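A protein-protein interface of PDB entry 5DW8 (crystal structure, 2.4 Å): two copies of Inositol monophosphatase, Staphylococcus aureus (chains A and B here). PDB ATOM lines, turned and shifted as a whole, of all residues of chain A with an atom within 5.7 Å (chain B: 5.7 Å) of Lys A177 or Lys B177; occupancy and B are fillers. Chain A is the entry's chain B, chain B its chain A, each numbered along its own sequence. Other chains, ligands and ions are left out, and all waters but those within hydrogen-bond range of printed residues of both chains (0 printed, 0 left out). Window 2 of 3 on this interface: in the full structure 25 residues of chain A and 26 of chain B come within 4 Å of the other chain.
OG1 of Thr B168 sits at hydrogen-bond distance from OD1 of Asn A181 (3.2 Å).
O of Lys B177 sits close to OD1 of Asn B181 (3.3 Å). The side-chain amino group (NZ) of Lys A177 is in salt-bridge range of the side-chain carboxylate (OE1) of Glu A174 (3.6 Å).
Among the printed residues, pairs that only touch across the chains: Leu A167 with Lys B177 (3.1 Å), Lys A177 with Thr B168 (3.5 Å), Lys A177 with Leu B167 (3.6 Å), Thr A168 with Lys B177 (3.6 Å), Thr A168 with Asn B181 (3.7 Å), Thr A168 with Leu B167 (3.8 Å), Lys A177 with Lys B177 (3.8 Å), Leu A167 with Leu B167 (3.9 Å) and Val A180 with Thr B168 (3.96 Å).
Ile A175 touches none of the printed residues of chain B. Lys A177 touches just these residues of chain B: Leu B167, Thr B168 and Lys B177. Printed residues of chain B within 4 Å of Asn A181: Thr B168. Of the printed residues of chain A, Thr B168 touches Lys A177, Val A180 and Asn A181. Of the printed residues of chain A, Lys B177 touches Leu A167, Thr A168 and Lys A177. The nearest printed residue of chain B that does not touch Lys A177 is Glu B174 (6.6 Å). The nearest printed residue of chain A that does not touch Lys B177 is Glu A174 (6.6 Å).
Printed residues of chain A that touch a printed residue of chain B: Leu A167, Thr A168, Lys A177, Val A180 and Asn A181. Hydrophobic or aromatic side chains of chain A within 4 Å of the printed part of chain B: Leu A167 and Val A180. Hydrophobic or aromatic side chains of chain B within 4 Å of the printed part of chain A: Leu B167. Along chain B the printed residues that touch a printed residue of chain A span positions 167 to 181. Among the printed residues, 10 pairs touch across the chains. Among the printed residues, no Asp or Glu carboxylate lies within 4 Å of a Lys or Arg side-chain nitrogen of the other chain.
Leu A167 touches Lys B177, and with the chains exchanged Lys A177 touches Leu B167. Thr A168 touches Lys B177, and with the chains exchanged Lys A177 touches Thr B168. Thr A168 touches Asn B181, and with the chains exchanged Asn A181 touches Thr B168. Lys B177 touches its own counterpart, Lys A177. Positions printed for both chains: 167, 168, 172, 173, 174, 175, 176, 177, 178, 179, 180, 181 and 182.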
ATOM      1  N   LEU A 167      13.125 -25.893 -16.091  1.00  0.00           N
ATOM      2  CA  LEU A 167      14.021 -26.273 -17.190  1.00  0.00           C
ATOM      3  C   LEU A 167      14.550 -25.034 -17.895  1.00  0.00           C
ATOM      4  O   LEU A 167      15.275 -25.155 -18.881  1.00  0.00           O
ATOM      5  CB  LEU A 167      13.304 -27.133 -18.232  1.00  0.00           C
ATOM      6  CG  LEU A 167      12.964 -28.582 -17.972  1.00  0.00           C
ATOM      7  CD1 LEU A 167      12.231 -28.756 -16.666  1.00  0.00           C
ATOM      8  CD2 LEU A 167      12.064 -29.003 -19.110  1.00  0.00           C
ATOM      9  N   THR A 168      14.138 -23.851 -17.436  1.00  0.00           N
ATOM     10  CA  THR A 168      14.589 -22.606 -18.031  1.00  0.00           C
ATOM     11  C   THR A 168      15.899 -22.161 -17.431  1.00  0.00           C
ATOM     12  O   THR A 168      16.653 -21.505 -18.098  1.00  0.00           O
ATOM     13  CB  THR A 168      13.583 -21.446 -17.846  1.00  0.00           C
ATOM     14  OG1 THR A 168      13.217 -21.359 -16.470  1.00  0.00           O
ATOM     15  CG2 THR A 168      12.364 -21.672 -18.670  1.00  0.00           C
ATOM     16  N   LEU A 172      20.588 -25.485 -13.304  1.00  0.00           N
ATOM     17  CA  LEU A 172      19.484 -26.351 -12.936  1.00  0.00           C
ATOM     18  C   LEU A 172      18.683 -26.927 -14.117  1.00  0.00           C
ATOM     19  O   LEU A 172      18.344 -28.108 -14.131  1.00  0.00           O
ATOM     20  CB  LEU A 172      18.551 -25.575 -12.047  1.00  0.00           C
ATOM     21  CG  LEU A 172      17.516 -26.414 -11.354  1.00  0.00           C
ATOM     22  CD1 LEU A 172      18.047 -27.734 -10.833  1.00  0.00           C
ATOM     23  CD2 LEU A 172      17.009 -25.568 -10.209  1.00  0.00           C
ATOM     24  N   GLY A 173      18.383 -26.104 -15.114  1.00  0.00           N
ATOM     25  CA  GLY A 173      17.728 -26.607 -16.315  1.00  0.00           C
ATOM     26  C   GLY A 173      18.453 -27.824 -16.913  1.00  0.00           C
ATOM     27  O   GLY A 173      17.831 -28.870 -17.166  1.00  0.00           O
ATOM     28  N   GLU A 174      19.768 -27.692 -17.106  1.00  0.00           N
ATOM     29  CA  GLU A 174      20.582 -28.766 -17.659  1.00  0.00           C
ATOM     30  C   GLU A 174      20.470 -30.075 -16.906  1.00  0.00           C
ATOM     31  O   GLU A 174      20.297 -31.131 -17.499  1.00  0.00           O
ATOM     32  CB  GLU A 174      22.065 -28.352 -17.692  1.00  0.00           C
ATOM     33  CG  GLU A 174      22.423 -27.579 -18.941  1.00  0.00           C
ATOM     34  CD  GLU A 174      21.965 -28.305 -20.192  1.00  0.00           C
ATOM     35  OE1 GLU A 174      21.460 -27.617 -21.106  1.00  0.00           O
ATOM     36  OE2 GLU A 174      22.070 -29.569 -20.239  1.00  0.00           O
ATOM     37  N   ILE A 175      20.630 -29.980 -15.601  1.00  0.00           N
ATOM     38  CA  ILE A 175      20.389 -31.085 -14.694  1.00  0.00           C
ATOM     39  C   ILE A 175      18.994 -31.698 -14.870  1.00  0.00           C
ATOM     40  O   ILE A 175      18.880 -32.918 -14.943  1.00  0.00           O
ATOM     41  CB  ILE A 175      20.598 -30.605 -13.256  1.00  0.00           C
ATOM     42  CG1 ILE A 175      22.084 -30.334 -13.061  1.00  0.00           C
ATOM     43  CG2 ILE A 175      20.067 -31.609 -12.253  1.00  0.00           C
ATOM     44  CD1 ILE A 175      22.469 -29.832 -11.695  1.00  0.00           C
ATOM     45  N   PHE A 176      17.944 -30.883 -14.972  1.00  0.00           N
ATOM     46  CA  PHE A 176      16.576 -31.447 -15.033  1.00  0.00           C
ATOM     47  C   PHE A 176      16.197 -31.897 -16.429  1.00  0.00           C
ATOM     48  O   PHE A 176      15.298 -32.722 -16.555  1.00  0.00           O
ATOM     49  CB  PHE A 176      15.484 -30.492 -14.519  1.00  0.00           C
ATOM     50  CG  PHE A 176      15.350 -30.432 -13.012  1.00  0.00           C
ATOM     51  CD1 PHE A 176      15.387 -31.576 -12.231  1.00  0.00           C
ATOM     52  CD2 PHE A 176      15.116 -29.221 -12.385  1.00  0.00           C
ATOM     53  CE1 PHE A 176      15.234 -31.506 -10.852  1.00  0.00           C
ATOM     54  CE2 PHE A 176      14.950 -29.139 -11.004  1.00  0.00           C
ATOM     55  CZ  PHE A 176      15.018 -30.285 -10.229  1.00  0.00           C
ATOM     56  N   LYS A 177      16.857 -31.365 -17.461  1.00  0.00           N
ATOM     57  CA  LYS A 177      16.648 -31.818 -18.844  1.00  0.00           C
ATOM     58  C   LYS A 177      16.911 -33.315 -18.971  1.00  0.00           C
ATOM     59  O   LYS A 177      16.154 -34.065 -19.603  1.00  0.00           O
ATOM     60  CB  LYS A 177      17.588 -31.090 -19.816  1.00  0.00           C
ATOM     61  CG  LYS A 177      16.962 -29.921 -20.583  1.00  0.00           C
ATOM     62  CD  LYS A 177      17.011 -28.573 -19.852  1.00  0.00           C
ATOM     63  CE  LYS A 177      16.793 -27.389 -20.778  1.00  0.00           C
ATOM     64  NZ  LYS A 177      17.913 -27.223 -21.745  1.00  0.00           N
ATOM     65  N   GLU A 178      18.033 -33.707 -18.378  1.00  0.00           N
ATOM     66  CA  GLU A 178      18.472 -35.083 -18.312  1.00  0.00           C
ATOM     67  C   GLU A 178      17.323 -35.931 -17.863  1.00  0.00           C
ATOM     68  O   GLU A 178      17.038 -36.932 -18.463  1.00  0.00           O
ATOM     69  CB  GLU A 178      19.602 -35.230 -17.301  1.00  0.00           C
ATOM     70  CG  GLU A 178      20.772 -36.015 -17.822  1.00  0.00           C
ATOM     71  CD  GLU A 178      21.383 -35.327 -18.993  1.00  0.00           C
ATOM     72  OE1 GLU A 178      20.717 -35.291 -20.036  1.00  0.00           O
ATOM     73  OE2 GLU A 178      22.514 -34.818 -18.853  1.00  0.00           O
ATOM     74  N   ILE A 179      16.629 -35.540 -16.802  1.00  0.00           N
ATOM     75  CA  ILE A 179      15.659 -36.496 -16.267  1.00  0.00           C
ATOM     76  C   ILE A 179      14.349 -36.439 -17.025  1.00  0.00           C
ATOM     77  O   ILE A 179      13.706 -37.481 -17.179  1.00  0.00           O
ATOM     78  CB  ILE A 179      15.448 -36.464 -14.727  1.00  0.00           C
ATOM     79  CG1 ILE A 179      14.091 -35.934 -14.369  1.00  0.00           C
ATOM     80  CG2 ILE A 179      16.533 -35.686 -14.023  1.00  0.00           C
ATOM     81  CD1 ILE A 179      13.324 -36.834 -13.444  1.00  0.00           C
ATOM     82  N   VAL A 180      14.004 -35.242 -17.513  1.00  0.00           N
ATOM     83  CA  VAL A 180      12.854 -35.014 -18.385  1.00  0.00           C
ATOM     84  C   VAL A 180      12.986 -35.840 -19.679  1.00  0.00           C
ATOM     85  O   VAL A 180      12.035 -36.522 -20.060  1.00  0.00           O
ATOM     86  CB  VAL A 180      12.681 -33.502 -18.734  1.00  0.00           C
ATOM     87  CG1 VAL A 180      11.640 -33.316 -19.844  1.00  0.00           C
ATOM     88  CG2 VAL A 180      12.324 -32.676 -17.495  1.00  0.00           C
ATOM     89  N   ASN A 181      14.152 -35.792 -20.346  1.00  0.00           N
ATOM     90  CA  ASN A 181      14.345 -36.586 -21.603  1.00  0.00           C
ATOM     91  C   ASN A 181      14.177 -38.084 -21.343  1.00  0.00           C
ATOM     92  O   ASN A 181      13.731 -38.852 -22.189  1.00  0.00           O
ATOM     93  CB  ASN A 181      15.719 -36.385 -22.220  1.00  0.00           C
ATOM     94  CG  ASN A 181      15.953 -34.973 -22.739  1.00  0.00           C
ATOM     95  OD1 ASN A 181      15.019 -34.189 -23.004  1.00  0.00           O
ATOM     96  ND2 ASN A 181      17.224 -34.651 -22.923  1.00  0.00           N
ATOM     97  N   ASP A 182      14.538 -38.483 -20.143  1.00  0.00           N
ATOM     98  CA  ASP A 182      14.550 -39.878 -19.787  1.00  0.00           C
ATOM     99  C   ASP A 182      13.195 -40.484 -19.459  1.00  0.00           C
ATOM    100  O   ASP A 182      12.912 -41.607 -19.811  1.00  0.00           O
ATOM    101  CB  ASP A 182      15.413 -40.005 -18.566  1.00  0.00           C
ATOM    102  CG  ASP A 182      16.302 -41.131 -18.662  1.00  0.00           C
ATOM    103  OD1 ASP A 182      17.500 -40.899 -19.009  1.00  0.00           O
ATOM    104  OD2 ASP A 182      15.762 -42.248 -18.431  1.00  0.00           O
ATOM    105  N   LEU B 167      10.937 -27.819 -23.887  1.00  0.00           N
ATOM    106  CA  LEU B 167      11.925 -26.879 -23.415  1.00  0.00           C
ATOM    107  C   LEU B 167      13.314 -27.460 -23.429  1.00  0.00           C
ATOM    108  O   LEU B 167      14.267 -26.757 -23.212  1.00  0.00           O
ATOM    109  CB  LEU B 167      11.593 -26.438 -21.985  1.00  0.00           C
ATOM    110  CG  LEU B 167      10.913 -25.095 -21.814  1.00  0.00           C
ATOM    111  CD1 LEU B 167       9.512 -25.118 -22.405  1.00  0.00           C
ATOM    112  CD2 LEU B 167      10.898 -24.774 -20.331  1.00  0.00           C
ATOM    113  N   THR B 168      13.436 -28.752 -23.660  1.00  0.00           N
ATOM    114  CA  THR B 168      14.743 -29.381 -23.780  1.00  0.00           C
ATOM    115  C   THR B 168      15.270 -29.289 -25.227  1.00  0.00           C
ATOM    116  O   THR B 168      16.424 -29.546 -25.481  1.00  0.00           O
ATOM    117  CB  THR B 168      14.651 -30.855 -23.396  1.00  0.00           C
ATOM    118  OG1 THR B 168      13.846 -31.518 -24.364  1.00  0.00           O
ATOM    119  CG2 THR B 168      14.012 -31.030 -22.037  1.00  0.00           C
ATOM    120  N   LEU B 172      13.889 -24.719 -30.436  1.00  0.00           N
ATOM    121  CA  LEU B 172      12.530 -24.599 -29.901  1.00  0.00           C
ATOM    122  C   LEU B 172      12.557 -24.190 -28.426  1.00  0.00           C
ATOM    123  O   LEU B 172      11.742 -23.376 -27.998  1.00  0.00           O
ATOM    124  CB  LEU B 172      11.777 -25.917 -30.101  1.00  0.00           C
ATOM    125  CG  LEU B 172      10.253 -25.892 -30.156  1.00  0.00           C
ATOM    126  CD1 LEU B 172       9.672 -24.862 -31.111  1.00  0.00           C
ATOM    127  CD2 LEU B 172       9.781 -27.282 -30.561  1.00  0.00           C
ATOM    128  N   GLY B 173      13.543 -24.727 -27.700  1.00  0.00           N
ATOM    129  CA  GLY B 173      13.780 -24.468 -26.278  1.00  0.00           C
ATOM    130  C   GLY B 173      13.979 -23.032 -25.851  1.00  0.00           C
ATOM    131  O   GLY B 173      13.276 -22.582 -24.960  1.00  0.00           O
ATOM    132  N   GLU B 174      14.907 -22.304 -26.483  1.00  0.00           N
ATOM    133  CA  GLU B 174      15.127 -20.866 -26.172  1.00  0.00           C
ATOM    134  C   GLU B 174      13.867 -20.077 -26.425  1.00  0.00           C
ATOM    135  O   GLU B 174      13.442 -19.256 -25.598  1.00  0.00           O
ATOM    136  CB  GLU B 174      16.252 -20.233 -27.006  1.00  0.00           C
ATOM    137  CG  GLU B 174      17.650 -20.769 -26.720  1.00  0.00           C
ATOM    138  CD  GLU B 174      18.103 -20.589 -25.270  1.00  0.00           C
ATOM    139  OE1 GLU B 174      18.817 -21.486 -24.777  1.00  0.00           O
ATOM    140  OE2 GLU B 174      17.765 -19.571 -24.620  1.00  0.00           O
ATOM    141  N   ILE B 175      13.261 -20.351 -27.571  1.00  0.00           N
ATOM    142  CA  ILE B 175      12.007 -19.722 -27.952  1.00  0.00           C
ATOM    143  C   ILE B 175      10.917 -19.914 -26.866  1.00  0.00           C
ATOM    144  O   ILE B 175      10.332 -18.939 -26.437  1.00  0.00           O
ATOM    145  CB  ILE B 175      11.531 -20.206 -29.341  1.00  0.00           C
ATOM    146  CG1 ILE B 175      12.609 -19.931 -30.394  1.00  0.00           C
ATOM    147  CG2 ILE B 175      10.231 -19.510 -29.728  1.00  0.00           C
ATOM    148  CD1 ILE B 175      12.426 -20.668 -31.712  1.00  0.00           C
ATOM    149  N   PHE B 176      10.663 -21.136 -26.407  1.00  0.00           N
ATOM    150  CA  PHE B 176       9.634 -21.356 -25.375  1.00  0.00           C
ATOM    151  C   PHE B 176      10.072 -20.924 -23.983  1.00  0.00           C
ATOM    152  O   PHE B 176       9.231 -20.648 -23.155  1.00  0.00           O
ATOM    153  CB  PHE B 176       9.178 -22.808 -25.331  1.00  0.00           C
ATOM    154  CG  PHE B 176       8.305 -23.226 -26.502  1.00  0.00           C
ATOM    155  CD1 PHE B 176       7.249 -22.436 -26.932  1.00  0.00           C
ATOM    156  CD2 PHE B 176       8.527 -24.415 -27.154  1.00  0.00           C
ATOM    157  CE1 PHE B 176       6.438 -22.822 -27.990  1.00  0.00           C
ATOM    158  CE2 PHE B 176       7.718 -24.807 -28.212  1.00  0.00           C
ATOM    159  CZ  PHE B 176       6.669 -24.009 -28.627  1.00  0.00           C
ATOM    160  N   LYS B 177      11.383 -20.856 -23.741  1.00  0.00           N
ATOM    161  CA  LYS B 177      11.947 -20.351 -22.503  1.00  0.00           C
ATOM    162  C   LYS B 177      11.469 -18.924 -22.212  1.00  0.00           C
ATOM    163  O   LYS B 177      10.889 -18.639 -21.144  1.00  0.00           O
ATOM    164  CB  LYS B 177      13.483 -20.362 -22.586  1.00  0.00           C
ATOM    165  CG  LYS B 177      14.225 -21.422 -21.750  1.00  0.00           C
ATOM    166  CD  LYS B 177      13.845 -22.879 -22.035  1.00  0.00           C
ATOM    167  CE  LYS B 177      14.959 -23.881 -21.677  1.00  0.00           C
ATOM    168  NZ  LYS B 177      16.223 -23.852 -22.487  1.00  0.00           N
ATOM    169  N   GLU B 178      11.724 -18.030 -23.168  1.00  0.00           N
ATOM    170  CA  GLU B 178      11.290 -16.648 -23.074  1.00  0.00           C
ATOM    171  C   GLU B 178       9.824 -16.593 -22.737  1.00  0.00           C
ATOM    172  O   GLU B 178       9.421 -15.806 -21.903  1.00  0.00           O
ATOM    173  CB  GLU B 178      11.532 -15.894 -24.376  1.00  0.00           C
ATOM    174  CG  GLU B 178      12.529 -14.761 -24.274  1.00  0.00           C
ATOM    175  CD  GLU B 178      13.965 -15.221 -24.390  1.00  0.00           C
ATOM    176  OE1 GLU B 178      14.734 -14.541 -25.102  1.00  0.00           O
ATOM    177  OE2 GLU B 178      14.339 -16.235 -23.766  1.00  0.00           O
ATOM    178  N   ILE B 179       9.005 -17.442 -23.368  1.00  0.00           N
ATOM    179  CA  ILE B 179       7.560 -17.332 -23.140  1.00  0.00           C
ATOM    180  C   ILE B 179       7.092 -18.034 -21.835  1.00  0.00           C
ATOM    181  O   ILE B 179       6.067 -17.653 -21.288  1.00  0.00           O
ATOM    182  CB  ILE B 179       6.674 -17.699 -24.367  1.00  0.00           C
ATOM    183  CG1 ILE B 179       5.817 -18.917 -24.093  1.00  0.00           C
ATOM    184  CG2 ILE B 179       7.442 -17.832 -25.668  1.00  0.00           C
ATOM    185  CD1 ILE B 179       4.365 -18.555 -23.758  1.00  0.00           C
ATOM    186  N   VAL B 180       7.853 -19.014 -21.327  1.00  0.00           N
ATOM    187  CA  VAL B 180       7.564 -19.602 -20.019  1.00  0.00           C
ATOM    188  C   VAL B 180       7.924 -18.600 -18.916  1.00  0.00           C
ATOM    189  O   VAL B 180       7.153 -18.430 -17.979  1.00  0.00           O
ATOM    190  CB  VAL B 180       8.290 -20.940 -19.803  1.00  0.00           C
ATOM    191  CG1 VAL B 180       8.080 -21.460 -18.387  1.00  0.00           C
ATOM    192  CG2 VAL B 180       7.793 -21.958 -20.801  1.00  0.00           C
ATOM    193  N   ASN B 181       9.088 -17.949 -19.056  1.00  0.00           N
ATOM    194  CA  ASN B 181       9.548 -16.882 -18.139  1.00  0.00           C
ATOM    195  C   ASN B 181       8.568 -15.757 -17.900  1.00  0.00           C
ATOM    196  O   ASN B 181       8.543 -15.161 -16.838  1.00  0.00           O
ATOM    197  CB  ASN B 181      10.810 -16.226 -18.687  1.00  0.00           C
ATOM    198  CG  ASN B 181      12.053 -16.800 -18.093  1.00  0.00           C
ATOM    199  OD1 ASN B 181      12.316 -17.985 -18.229  1.00  0.00           O
ATOM    200  ND2 ASN B 181      12.827 -15.961 -17.390  1.00  0.00           N
ATOM    201  N   ASP B 182       7.817 -15.415 -18.925  1.00  0.00           N
ATOM    202  CA  ASP B 182       6.894 -14.309 -18.822  1.00  0.00           C
ATOM    203  C   ASP B 182       5.511 -14.695 -18.353  1.00  0.00           C
ATOM    204  O   ASP B 182       4.900 -13.984 -17.588  1.00  0.00           O
ATOM    205  CB  ASP B 182       6.805 -13.607 -20.146  1.00  0.00           C
ATOM    206  CG  ASP B 182       7.667 -12.443 -20.172  1.00  0.00           C
ATOM    207  OD1 ASP B 182       8.788 -12.537 -20.691  1.00  0.00           O
ATOM    208  OD2 ASP B 182       7.223 -11.445 -19.576  1.00  0.00           O
